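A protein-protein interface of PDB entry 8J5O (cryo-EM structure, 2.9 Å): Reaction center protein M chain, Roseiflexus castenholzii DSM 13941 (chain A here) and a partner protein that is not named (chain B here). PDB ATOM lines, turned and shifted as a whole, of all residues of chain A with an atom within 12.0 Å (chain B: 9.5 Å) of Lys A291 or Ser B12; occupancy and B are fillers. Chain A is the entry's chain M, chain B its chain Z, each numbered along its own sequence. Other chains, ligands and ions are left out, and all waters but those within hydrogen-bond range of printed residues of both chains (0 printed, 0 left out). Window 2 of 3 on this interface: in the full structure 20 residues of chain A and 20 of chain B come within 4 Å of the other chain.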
ATOM      1  N   TYR A 186       4.891   0.831 -22.987  1.00  0.00           N
ATOM      2  CA  TYR A 186       3.976   0.920 -21.858  1.00  0.00           C
ATOM      3  C   TYR A 186       4.014   2.295 -21.204  1.00  0.00           C
ATOM      4  O   TYR A 186       3.044   2.680 -20.546  1.00  0.00           O
ATOM      5  CB  TYR A 186       4.284  -0.162 -20.825  1.00  0.00           C
ATOM      6  CG  TYR A 186       3.735  -1.520 -21.187  1.00  0.00           C
ATOM      7  CD1 TYR A 186       2.436  -1.660 -21.652  1.00  0.00           C
ATOM      8  CD2 TYR A 186       4.518  -2.657 -21.084  1.00  0.00           C
ATOM      9  CE1 TYR A 186       1.929  -2.895 -21.991  1.00  0.00           C
ATOM     10  CE2 TYR A 186       4.019  -3.897 -21.421  1.00  0.00           C
ATOM     11  CZ  TYR A 186       2.724  -4.011 -21.874  1.00  0.00           C
ATOM     12  OH  TYR A 186       2.223  -5.244 -22.212  1.00  0.00           O
ATOM     13  N   TYR A 187       5.106   3.043 -21.370  1.00  0.00           N
ATOM     14  CA  TYR A 187       5.221   4.398 -20.850  1.00  0.00           C
ATOM     15  C   TYR A 187       5.090   5.450 -21.945  1.00  0.00           C
ATOM     16  O   TYR A 187       5.441   6.613 -21.729  1.00  0.00           O
ATOM     17  CB  TYR A 187       6.536   4.552 -20.092  1.00  0.00           C
ATOM     18  CG  TYR A 187       6.542   3.743 -18.821  1.00  0.00           C
ATOM     19  CD1 TYR A 187       5.872   4.188 -17.690  1.00  0.00           C
ATOM     20  CD2 TYR A 187       7.181   2.515 -18.761  1.00  0.00           C
ATOM     21  CE1 TYR A 187       5.858   3.444 -16.530  1.00  0.00           C
ATOM     22  CE2 TYR A 187       7.173   1.763 -17.606  1.00  0.00           C
ATOM     23  CZ  TYR A 187       6.511   2.232 -16.494  1.00  0.00           C
ATOM     24  OH  TYR A 187       6.502   1.487 -15.340  1.00  0.00           O
ATOM     25  N   PRO A 189       2.607   7.785 -23.692  1.00  0.00           N
ATOM     26  CA  PRO A 189       1.237   8.253 -23.411  1.00  0.00           C
ATOM     27  C   PRO A 189       0.267   8.036 -24.559  1.00  0.00           C
ATOM     28  O   PRO A 189      -0.924   7.783 -24.327  1.00  0.00           O
ATOM     29  CB  PRO A 189       1.436   9.745 -23.108  1.00  0.00           C
ATOM     30  CG  PRO A 189       2.870   9.879 -22.743  1.00  0.00           C
ATOM     31  CD  PRO A 189       3.598   8.864 -23.560  1.00  0.00           C
ATOM     32  N   MET A 192      -0.916   4.587 -24.551  1.00  0.00           N
ATOM     33  CA  MET A 192      -1.956   4.458 -23.536  1.00  0.00           C
ATOM     34  C   MET A 192      -3.303   4.949 -24.056  1.00  0.00           C
ATOM     35  O   MET A 192      -4.336   4.297 -23.856  1.00  0.00           O
ATOM     36  CB  MET A 192      -1.559   5.231 -22.278  1.00  0.00           C
ATOM     37  CG  MET A 192      -0.317   4.713 -21.580  1.00  0.00           C
ATOM     38  SD  MET A 192       0.055   5.641 -20.080  1.00  0.00           S
ATOM     39  CE  MET A 192       1.693   6.255 -20.443  1.00  0.00           C
ATOM     40  N   ASP A 282      13.919   7.469 -25.393  1.00  0.00           N
ATOM     41  CA  ASP A 282      13.754   6.492 -24.319  1.00  0.00           C
ATOM     42  C   ASP A 282      12.504   6.872 -23.537  1.00  0.00           C
ATOM     43  O   ASP A 282      12.466   7.929 -22.901  1.00  0.00           O
ATOM     44  CB  ASP A 282      14.989   6.461 -23.417  1.00  0.00           C
ATOM     45  CG  ASP A 282      14.991   5.289 -22.451  1.00  0.00           C
ATOM     46  OD1 ASP A 282      13.909   4.766 -22.114  1.00  0.00           O
ATOM     47  OD2 ASP A 282      16.092   4.884 -22.029  1.00  0.00           O
ATOM     48  N   TRP A 283      11.486   6.012 -23.587  1.00  0.00           N
ATOM     49  CA  TRP A 283      10.201   6.323 -22.969  1.00  0.00           C
ATOM     50  C   TRP A 283      10.225   6.125 -21.456  1.00  0.00           C
ATOM     51  O   TRP A 283       9.547   6.853 -20.725  1.00  0.00           O
ATOM     52  CB  TRP A 283       9.106   5.474 -23.612  1.00  0.00           C
ATOM     53  CG  TRP A 283       8.609   6.042 -24.908  1.00  0.00           C
ATOM     54  CD1 TRP A 283       8.586   5.418 -26.118  1.00  0.00           C
ATOM     55  CD2 TRP A 283       8.044   7.342 -25.117  1.00  0.00           C
ATOM     56  NE1 TRP A 283       8.057   6.252 -27.071  1.00  0.00           N
ATOM     57  CE2 TRP A 283       7.714   7.439 -26.481  1.00  0.00           C
ATOM     58  CE3 TRP A 283       7.788   8.434 -24.283  1.00  0.00           C
ATOM     59  CZ2 TRP A 283       7.142   8.584 -27.031  1.00  0.00           C
ATOM     60  CZ3 TRP A 283       7.220   9.567 -24.830  1.00  0.00           C
ATOM     61  CH2 TRP A 283       6.904   9.633 -26.190  1.00  0.00           C
ATOM     62  N   TYR A 284      10.989   5.145 -20.966  1.00  0.00           N
ATOM     63  CA  TYR A 284      11.066   4.929 -19.523  1.00  0.00           C
ATOM     64  C   TYR A 284      11.761   6.094 -18.829  1.00  0.00           C
ATOM     65  O   TYR A 284      11.337   6.519 -17.749  1.00  0.00           O
ATOM     66  CB  TYR A 284      11.759   3.589 -19.238  1.00  0.00           C
ATOM     67  CG  TYR A 284      12.018   3.249 -17.774  1.00  0.00           C
ATOM     68  CD1 TYR A 284      13.089   3.798 -17.075  1.00  0.00           C
ATOM     69  CD2 TYR A 284      11.165   2.397 -17.086  1.00  0.00           C
ATOM     70  CE1 TYR A 284      13.311   3.493 -15.753  1.00  0.00           C
ATOM     71  CE2 TYR A 284      11.381   2.090 -15.760  1.00  0.00           C
ATOM     72  CZ  TYR A 284      12.456   2.641 -15.099  1.00  0.00           C
ATOM     73  OH  TYR A 284      12.683   2.342 -13.778  1.00  0.00           O
ATOM     74  N   ALA A 285      12.838   6.614 -19.422  1.00  0.00           N
ATOM     75  CA  ALA A 285      13.516   7.763 -18.833  1.00  0.00           C
ATOM     76  C   ALA A 285      12.610   8.988 -18.817  1.00  0.00           C
ATOM     77  O   ALA A 285      12.583   9.742 -17.834  1.00  0.00           O
ATOM     78  CB  ALA A 285      14.808   8.054 -19.595  1.00  0.00           C
ATOM     79  N   TRP A 286      11.855   9.200 -19.897  1.00  0.00           N
ATOM     80  CA  TRP A 286      10.897  10.298 -19.924  1.00  0.00           C
ATOM     81  C   TRP A 286       9.840  10.125 -18.843  1.00  0.00           C
ATOM     82  O   TRP A 286       9.479  11.090 -18.158  1.00  0.00           O
ATOM     83  CB  TRP A 286      10.244  10.395 -21.304  1.00  0.00           C
ATOM     84  CG  TRP A 286       9.178  11.447 -21.391  1.00  0.00           C
ATOM     85  CD1 TRP A 286       9.346  12.754 -21.736  1.00  0.00           C
ATOM     86  CD2 TRP A 286       7.779  11.280 -21.125  1.00  0.00           C
ATOM     87  NE1 TRP A 286       8.144  13.412 -21.697  1.00  0.00           N
ATOM     88  CE2 TRP A 286       7.166  12.529 -21.325  1.00  0.00           C
ATOM     89  CE3 TRP A 286       6.990  10.195 -20.732  1.00  0.00           C
ATOM     90  CZ2 TRP A 286       5.799  12.724 -21.149  1.00  0.00           C
ATOM     91  CZ3 TRP A 286       5.635  10.392 -20.558  1.00  0.00           C
ATOM     92  CH2 TRP A 286       5.053  11.646 -20.766  1.00  0.00           C
ATOM     93  N   GLY A 287       9.327   8.905 -18.675  1.00  0.00           N
ATOM     94  CA  GLY A 287       8.339   8.666 -17.637  1.00  0.00           C
ATOM     95  C   GLY A 287       8.889   8.906 -16.244  1.00  0.00           C
ATOM     96  O   GLY A 287       8.187   9.416 -15.369  1.00  0.00           O
ATOM     97  N   GLU A 288      10.149   8.530 -16.019  1.00  0.00           N
ATOM     98  CA  GLU A 288      10.783   8.815 -14.736  1.00  0.00           C
ATOM     99  C   GLU A 288      10.895  10.316 -14.501  1.00  0.00           C
ATOM    100  O   GLU A 288      10.644  10.799 -13.392  1.00  0.00           O
ATOM    101  CB  GLU A 288      12.163   8.163 -14.670  1.00  0.00           C
ATOM    102  CG  GLU A 288      12.160   6.753 -14.121  1.00  0.00           C
ATOM    103  CD  GLU A 288      13.554   6.262 -13.794  1.00  0.00           C
ATOM    104  OE1 GLU A 288      14.487   6.559 -14.570  1.00  0.00           O
ATOM    105  OE2 GLU A 288      13.720   5.579 -12.762  1.00  0.00           O
ATOM    106  N   THR A 289      11.276  11.069 -15.534  1.00  0.00           N
ATOM    107  CA  THR A 289      11.356  12.518 -15.395  1.00  0.00           C
ATOM    108  C   THR A 289       9.985  13.170 -15.256  1.00  0.00           C
ATOM    109  O   THR A 289       9.898  14.295 -14.757  1.00  0.00           O
ATOM    110  CB  THR A 289      12.099  13.129 -16.583  1.00  0.00           C
ATOM    111  OG1 THR A 289      11.323  12.960 -17.774  1.00  0.00           O
ATOM    112  CG2 THR A 289      13.449  12.461 -16.763  1.00  0.00           C
ATOM    113  N   ALA A 290       8.918  12.498 -15.689  1.00  0.00           N
ATOM    114  CA  ALA A 290       7.569  13.042 -15.607  1.00  0.00           C
ATOM    115  C   ALA A 290       6.823  12.621 -14.347  1.00  0.00           C
ATOM    116  O   ALA A 290       5.674  13.035 -14.164  1.00  0.00           O
ATOM    117  CB  ALA A 290       6.757  12.629 -16.837  1.00  0.00           C
ATOM    118  N   LYS A 291       7.441  11.812 -13.485  1.00  0.00           N
ATOM    119  CA  LYS A 291       6.847  11.394 -12.212  1.00  0.00           C
ATOM    120  C   LYS A 291       5.629  10.492 -12.416  1.00  0.00           C
ATOM    121  O   LYS A 291       4.690  10.512 -11.620  1.00  0.00           O
ATOM    122  CB  LYS A 291       6.481  12.602 -11.345  1.00  0.00           C
ATOM    123  CG  LYS A 291       7.540  13.691 -11.298  1.00  0.00           C
ATOM    124  CD  LYS A 291       8.633  13.365 -10.300  1.00  0.00           C
ATOM    125  CE  LYS A 291       9.934  14.050 -10.676  1.00  0.00           C
ATOM    126  NZ  LYS A 291      11.041  13.691  -9.751  1.00  0.00           N
ATOM    127  N   ILE A 292       5.639   9.693 -13.480  1.00  0.00           N
ATOM    128  CA  ILE A 292       4.580   8.725 -13.731  1.00  0.00           C
ATOM    129  C   ILE A 292       5.098   7.292 -13.623  1.00  0.00           C
ATOM    130  O   ILE A 292       4.485   6.371 -14.142  1.00  0.00           O
ATOM    131  CB  ILE A 292       3.905   8.969 -15.094  1.00  0.00           C
ATOM    132  CG1 ILE A 292       4.841   8.569 -16.236  1.00  0.00           C
ATOM    133  CG2 ILE A 292       3.470  10.417 -15.226  1.00  0.00           C
ATOM    134  CD1 ILE A 292       4.162   8.485 -17.581  1.00  0.00           C
ATOM    135  N   VAL A 293       6.230   7.102 -12.951  1.00  0.00           N
ATOM    136  CA  VAL A 293       6.846   5.795 -12.768  1.00  0.00           C
ATOM    137  C   VAL A 293       6.902   5.503 -11.274  1.00  0.00           C
ATOM    138  O   VAL A 293       7.439   6.304 -10.500  1.00  0.00           O
ATOM    139  CB  VAL A 293       8.251   5.741 -13.394  1.00  0.00           C
ATOM    140  CG1 VAL A 293       9.004   4.527 -12.906  1.00  0.00           C
ATOM    141  CG2 VAL A 293       8.154   5.728 -14.910  1.00  0.00           C
ATOM    142  N   ALA A 294       6.342   4.365 -10.874  1.00  0.00           N
ATOM    143  CA  ALA A 294       6.247   3.995  -9.468  1.00  0.00           C
ATOM    144  C   ALA A 294       7.604   3.536  -8.937  1.00  0.00           C
ATOM    145  O   ALA A 294       8.326   2.810  -9.625  1.00  0.00           O
ATOM    146  CB  ALA A 294       5.217   2.887  -9.275  1.00  0.00           C
ATOM    147  N   PRO A 295       7.975   3.945  -7.724  1.00  0.00           N
ATOM    148  CA  PRO A 295       9.205   3.425  -7.117  1.00  0.00           C
ATOM    149  C   PRO A 295       9.113   1.926  -6.876  1.00  0.00           C
ATOM    150  O   PRO A 295       8.035   1.372  -6.657  1.00  0.00           O
ATOM    151  CB  PRO A 295       9.307   4.201  -5.799  1.00  0.00           C
ATOM    152  CG  PRO A 295       8.496   5.431  -6.022  1.00  0.00           C
ATOM    153  CD  PRO A 295       7.369   5.012  -6.914  1.00  0.00           C
ATOM    154  N   TRP A 296      10.268   1.275  -6.910  1.00  0.00           N
ATOM    155  CA  TRP A 296      10.344  -0.180  -6.922  1.00  0.00           C
ATOM    156  C   TRP A 296      11.661  -0.645  -6.306  1.00  0.00           C
ATOM    157  O   TRP A 296      12.486  -1.273  -6.980  1.00  0.00           O
ATOM    158  CB  TRP A 296      10.137  -0.645  -8.368  1.00  0.00           C
ATOM    159  CG  TRP A 296      10.113  -2.111  -8.639  1.00  0.00           C
ATOM    160  CD1 TRP A 296      11.115  -2.853  -9.190  1.00  0.00           C
ATOM    161  CD2 TRP A 296       9.062  -3.029  -8.326  1.00  0.00           C
ATOM    162  NE1 TRP A 296      10.733  -4.164  -9.289  1.00  0.00           N
ATOM    163  CE2 TRP A 296       9.482  -4.303  -8.751  1.00  0.00           C
ATOM    164  CE3 TRP A 296       7.805  -2.897  -7.740  1.00  0.00           C
ATOM    165  CZ2 TRP A 296       8.688  -5.436  -8.605  1.00  0.00           C
ATOM    166  CZ3 TRP A 296       7.019  -4.021  -7.597  1.00  0.00           C
ATOM    167  CH2 TRP A 296       7.463  -5.274  -8.028  1.00  0.00           C
ATOM    168  N   SER B  12      13.946  19.179  -7.119  1.00  0.00           N
ATOM    169  CA  SER B  12      13.141  19.065  -8.329  1.00  0.00           C
ATOM    170  C   SER B  12      11.895  18.218  -8.092  1.00  0.00           C
ATOM    171  O   SER B  12      11.801  17.094  -8.584  1.00  0.00           O
ATOM    172  CB  SER B  12      13.972  18.466  -9.467  1.00  0.00           C
ATOM    173  OG  SER B  12      13.200  18.317 -10.645  1.00  0.00           O
ATOM    174  N   PRO B  13      10.935  18.756  -7.332  1.00  0.00           N
ATOM    175  CA  PRO B  13       9.694  18.012  -7.071  1.00  0.00           C
ATOM    176  C   PRO B  13       8.711  18.020  -8.229  1.00  0.00           C
ATOM    177  O   PRO B  13       7.681  17.343  -8.141  1.00  0.00           O
ATOM    178  CB  PRO B  13       9.099  18.739  -5.850  1.00  0.00           C
ATOM    179  CG  PRO B  13      10.177  19.674  -5.358  1.00  0.00           C
ATOM    180  CD  PRO B  13      10.993  20.005  -6.561  1.00  0.00           C
ATOM    181  N   TRP B  14       8.988  18.756  -9.311  1.00  0.00           N
ATOM    182  CA  TRP B  14       8.007  18.939 -10.368  1.00  0.00           C
ATOM    183  C   TRP B  14       8.395  18.177 -11.631  1.00  0.00           C
ATOM    184  O   TRP B  14       9.582  17.965 -11.902  1.00  0.00           O
ATOM    185  CB  TRP B  14       7.843  20.423 -10.714  1.00  0.00           C
ATOM    186  CG  TRP B  14       7.947  21.334  -9.534  1.00  0.00           C
ATOM    187  CD1 TRP B  14       8.931  22.243  -9.286  1.00  0.00           C
ATOM    188  CD2 TRP B  14       7.031  21.426  -8.440  1.00  0.00           C
ATOM    189  NE1 TRP B  14       8.686  22.895  -8.105  1.00  0.00           N
ATOM    190  CE2 TRP B  14       7.524  22.412  -7.565  1.00  0.00           C
ATOM    191  CE3 TRP B  14       5.840  20.771  -8.115  1.00  0.00           C
ATOM    192  CZ2 TRP B  14       6.869  22.759  -6.388  1.00  0.00           C
ATOM    193  CZ3 TRP B  14       5.192  21.116  -6.948  1.00  0.00           C
ATOM    194  CH2 TRP B  14       5.707  22.101  -6.098  1.00  0.00           C
ATOM    195  N   PRO B  15       7.415  17.756 -12.423  1.00  0.00           N
ATOM    196  CA  PRO B  15       7.715  17.117 -13.710  1.00  0.00           C
ATOM    197  C   PRO B  15       8.234  18.128 -14.722  1.00  0.00           C
ATOM    198  O   PRO B  15       8.239  19.339 -14.499  1.00  0.00           O
ATOM    199  CB  PRO B  15       6.367  16.536 -14.149  1.00  0.00           C
ATOM    200  CG  PRO B  15       5.491  16.584 -12.934  1.00  0.00           C
ATOM    201  CD  PRO B  15       5.977  17.729 -12.115  1.00  0.00           C
ATOM    202  N   VAL B  16       8.682  17.601 -15.860  1.00  0.00           N
ATOM    203  CA  VAL B  16       9.135  18.453 -16.951  1.00  0.00           C
ATOM    204  C   VAL B  16       7.935  18.956 -17.747  1.00  0.00           C
ATOM    205  O   VAL B  16       6.822  18.436 -17.644  1.00  0.00           O
ATOM    206  CB  VAL B  16      10.136  17.707 -17.853  1.00  0.00           C
ATOM    207  CG1 VAL B  16      11.488  17.605 -17.169  1.00  0.00           C
ATOM    208  CG2 VAL B  16       9.609  16.327 -18.206  1.00  0.00           C
ATOM    209  N   SER B  18       7.337  18.842 -20.965  1.00  0.00           N
ATOM    210  CA  SER B  18       6.845  17.866 -21.930  1.00  0.00           C
ATOM    211  C   SER B  18       5.963  16.832 -21.250  1.00  0.00           C
ATOM    212  O   SER B  18       4.941  16.415 -21.806  1.00  0.00           O
ATOM    213  CB  SER B  18       8.016  17.197 -22.645  1.00  0.00           C
ATOM    214  OG  SER B  18       8.782  16.418 -21.747  1.00  0.00           O
ATOM    215  N   GLY B  19       6.346  16.403 -20.047  1.00  0.00           N
ATOM    216  CA  GLY B  19       5.479  15.528 -19.278  1.00  0.00           C
ATOM    217  C   GLY B  19       4.136  16.169 -18.997  1.00  0.00           C
ATOM    218  O   GLY B  19       3.088  15.556 -19.214  1.00  0.00           O
ATOM    219  N   TYR B  20       4.158  17.429 -18.546  1.00  0.00           N
ATOM    220  CA  TYR B  20       2.948  18.212 -18.310  1.00  0.00           C
ATOM    221  C   TYR B  20       2.006  18.159 -19.501  1.00  0.00           C
ATOM    222  O   TYR B  20       0.886  17.648 -19.396  1.00  0.00           O
ATOM    223  CB  TYR B  20       3.310  19.669 -17.997  1.00  0.00           C
ATOM    224  CG  TYR B  20       3.719  19.924 -16.568  1.00  0.00           C
ATOM    225  CD1 TYR B  20       2.860  19.634 -15.519  1.00  0.00           C
ATOM    226  CD2 TYR B  20       4.958  20.466 -16.269  1.00  0.00           C
ATOM    227  CE1 TYR B  20       3.228  19.868 -14.213  1.00  0.00           C
ATOM    228  CE2 TYR B  20       5.334  20.703 -14.966  1.00  0.00           C
ATOM    229  CZ  TYR B  20       4.466  20.404 -13.941  1.00  0.00           C
ATOM    230  OH  TYR B  20       4.838  20.642 -12.639  1.00  0.00           O
ATOM    231  N   CYS B  23       1.066  14.345 -20.957  1.00  0.00           N
ATOM    232  CA  CYS B  23       0.298  13.481 -20.071  1.00  0.00           C
ATOM    233  C   CYS B  23      -0.971  14.166 -19.574  1.00  0.00           C
ATOM    234  O   CYS B  23      -2.073  13.639 -19.747  1.00  0.00           O
ATOM    235  CB  CYS B  23       1.172  13.031 -18.895  1.00  0.00           C
ATOM    236  SG  CYS B  23       0.363  11.893 -17.752  1.00  0.00           S
ATOM    237  N   PHE B  24      -0.835  15.341 -18.954  1.00  0.00           N
ATOM    238  CA  PHE B  24      -1.954  15.908 -18.221  1.00  0.00           C
ATOM    239  C   PHE B  24      -2.869  16.776 -19.075  1.00  0.00           C
ATOM    240  O   PHE B  24      -3.969  17.101 -18.617  1.00  0.00           O
ATOM    241  CB  PHE B  24      -1.428  16.710 -17.031  1.00  0.00           C
ATOM    242  CG  PHE B  24      -0.356  16.000 -16.256  1.00  0.00           C
ATOM    243  CD1 PHE B  24      -0.636  14.826 -15.579  1.00  0.00           C
ATOM    244  CD2 PHE B  24       0.935  16.493 -16.219  1.00  0.00           C
ATOM    245  CE1 PHE B  24       0.349  14.166 -14.872  1.00  0.00           C
ATOM    246  CE2 PHE B  24       1.923  15.835 -15.513  1.00  0.00           C
ATOM    247  CZ  PHE B  24       1.630  14.671 -14.840  1.00  0.00           C
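Of chain B, only Ser B12 and Pro B15 come within 4 Å of Lys A291. No residue of chain A comes within 4 Å of Pro B13. Trp B14 touches none of the printed residues of chain A. Pro B15 touches three residues of chain A. Of the printed residues of chain A, Ser B18 touches Trp A286. Of the printed residues of chain A, Gly B19 touches Trp A286 (3.4 Å) and Ala A290 (3.999 Å). Glu A288 touches none of the printed residues of chain B. The nearest residue of chain B that does not touch Lys A291 is Trp B14 (4.1 Å). The nearest printed residue of chain B that does not touch Trp A286 is Cys B23 (4.5 Å).
NE1 of Trp A286 lies within hydrogen-bond range of OG of Ser B18 (3.1 Å).
Among the printed residues, merely in contact across the chains: Trp A286 with Gly B19 (3.4 Å), Ala A290 with Pro B15 (3.6 Å), Lys A291 with Ser B12 (3.7 Å), Thr A289 with Val B16 (3.7 Å), Thr A289 with Pro B15 (3.7 Å), Lys A291 with Pro B15 (3.9 Å) and Ala A290 with Gly B19 (3.999 Å).
Hydrophobic or aromatic side chains of chain B within 4 Å of the printed part of chain A: Pro B15 and Val B16. Of the 19 printed residues of chain A, 4 touch a printed residue of chain B. Along chain A the printed residues that touch a printed residue of chain B span positions 286 to 291.
O of Ala A285 lies close to OG1 of Thr A289 (3.5 Å). The backbone carbonyl oxygen (O) of Trp A286 sits at hydrogen-bond distance from the side-chain hydroxyl (OG1) of Thr A289, 2.7 Å away.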
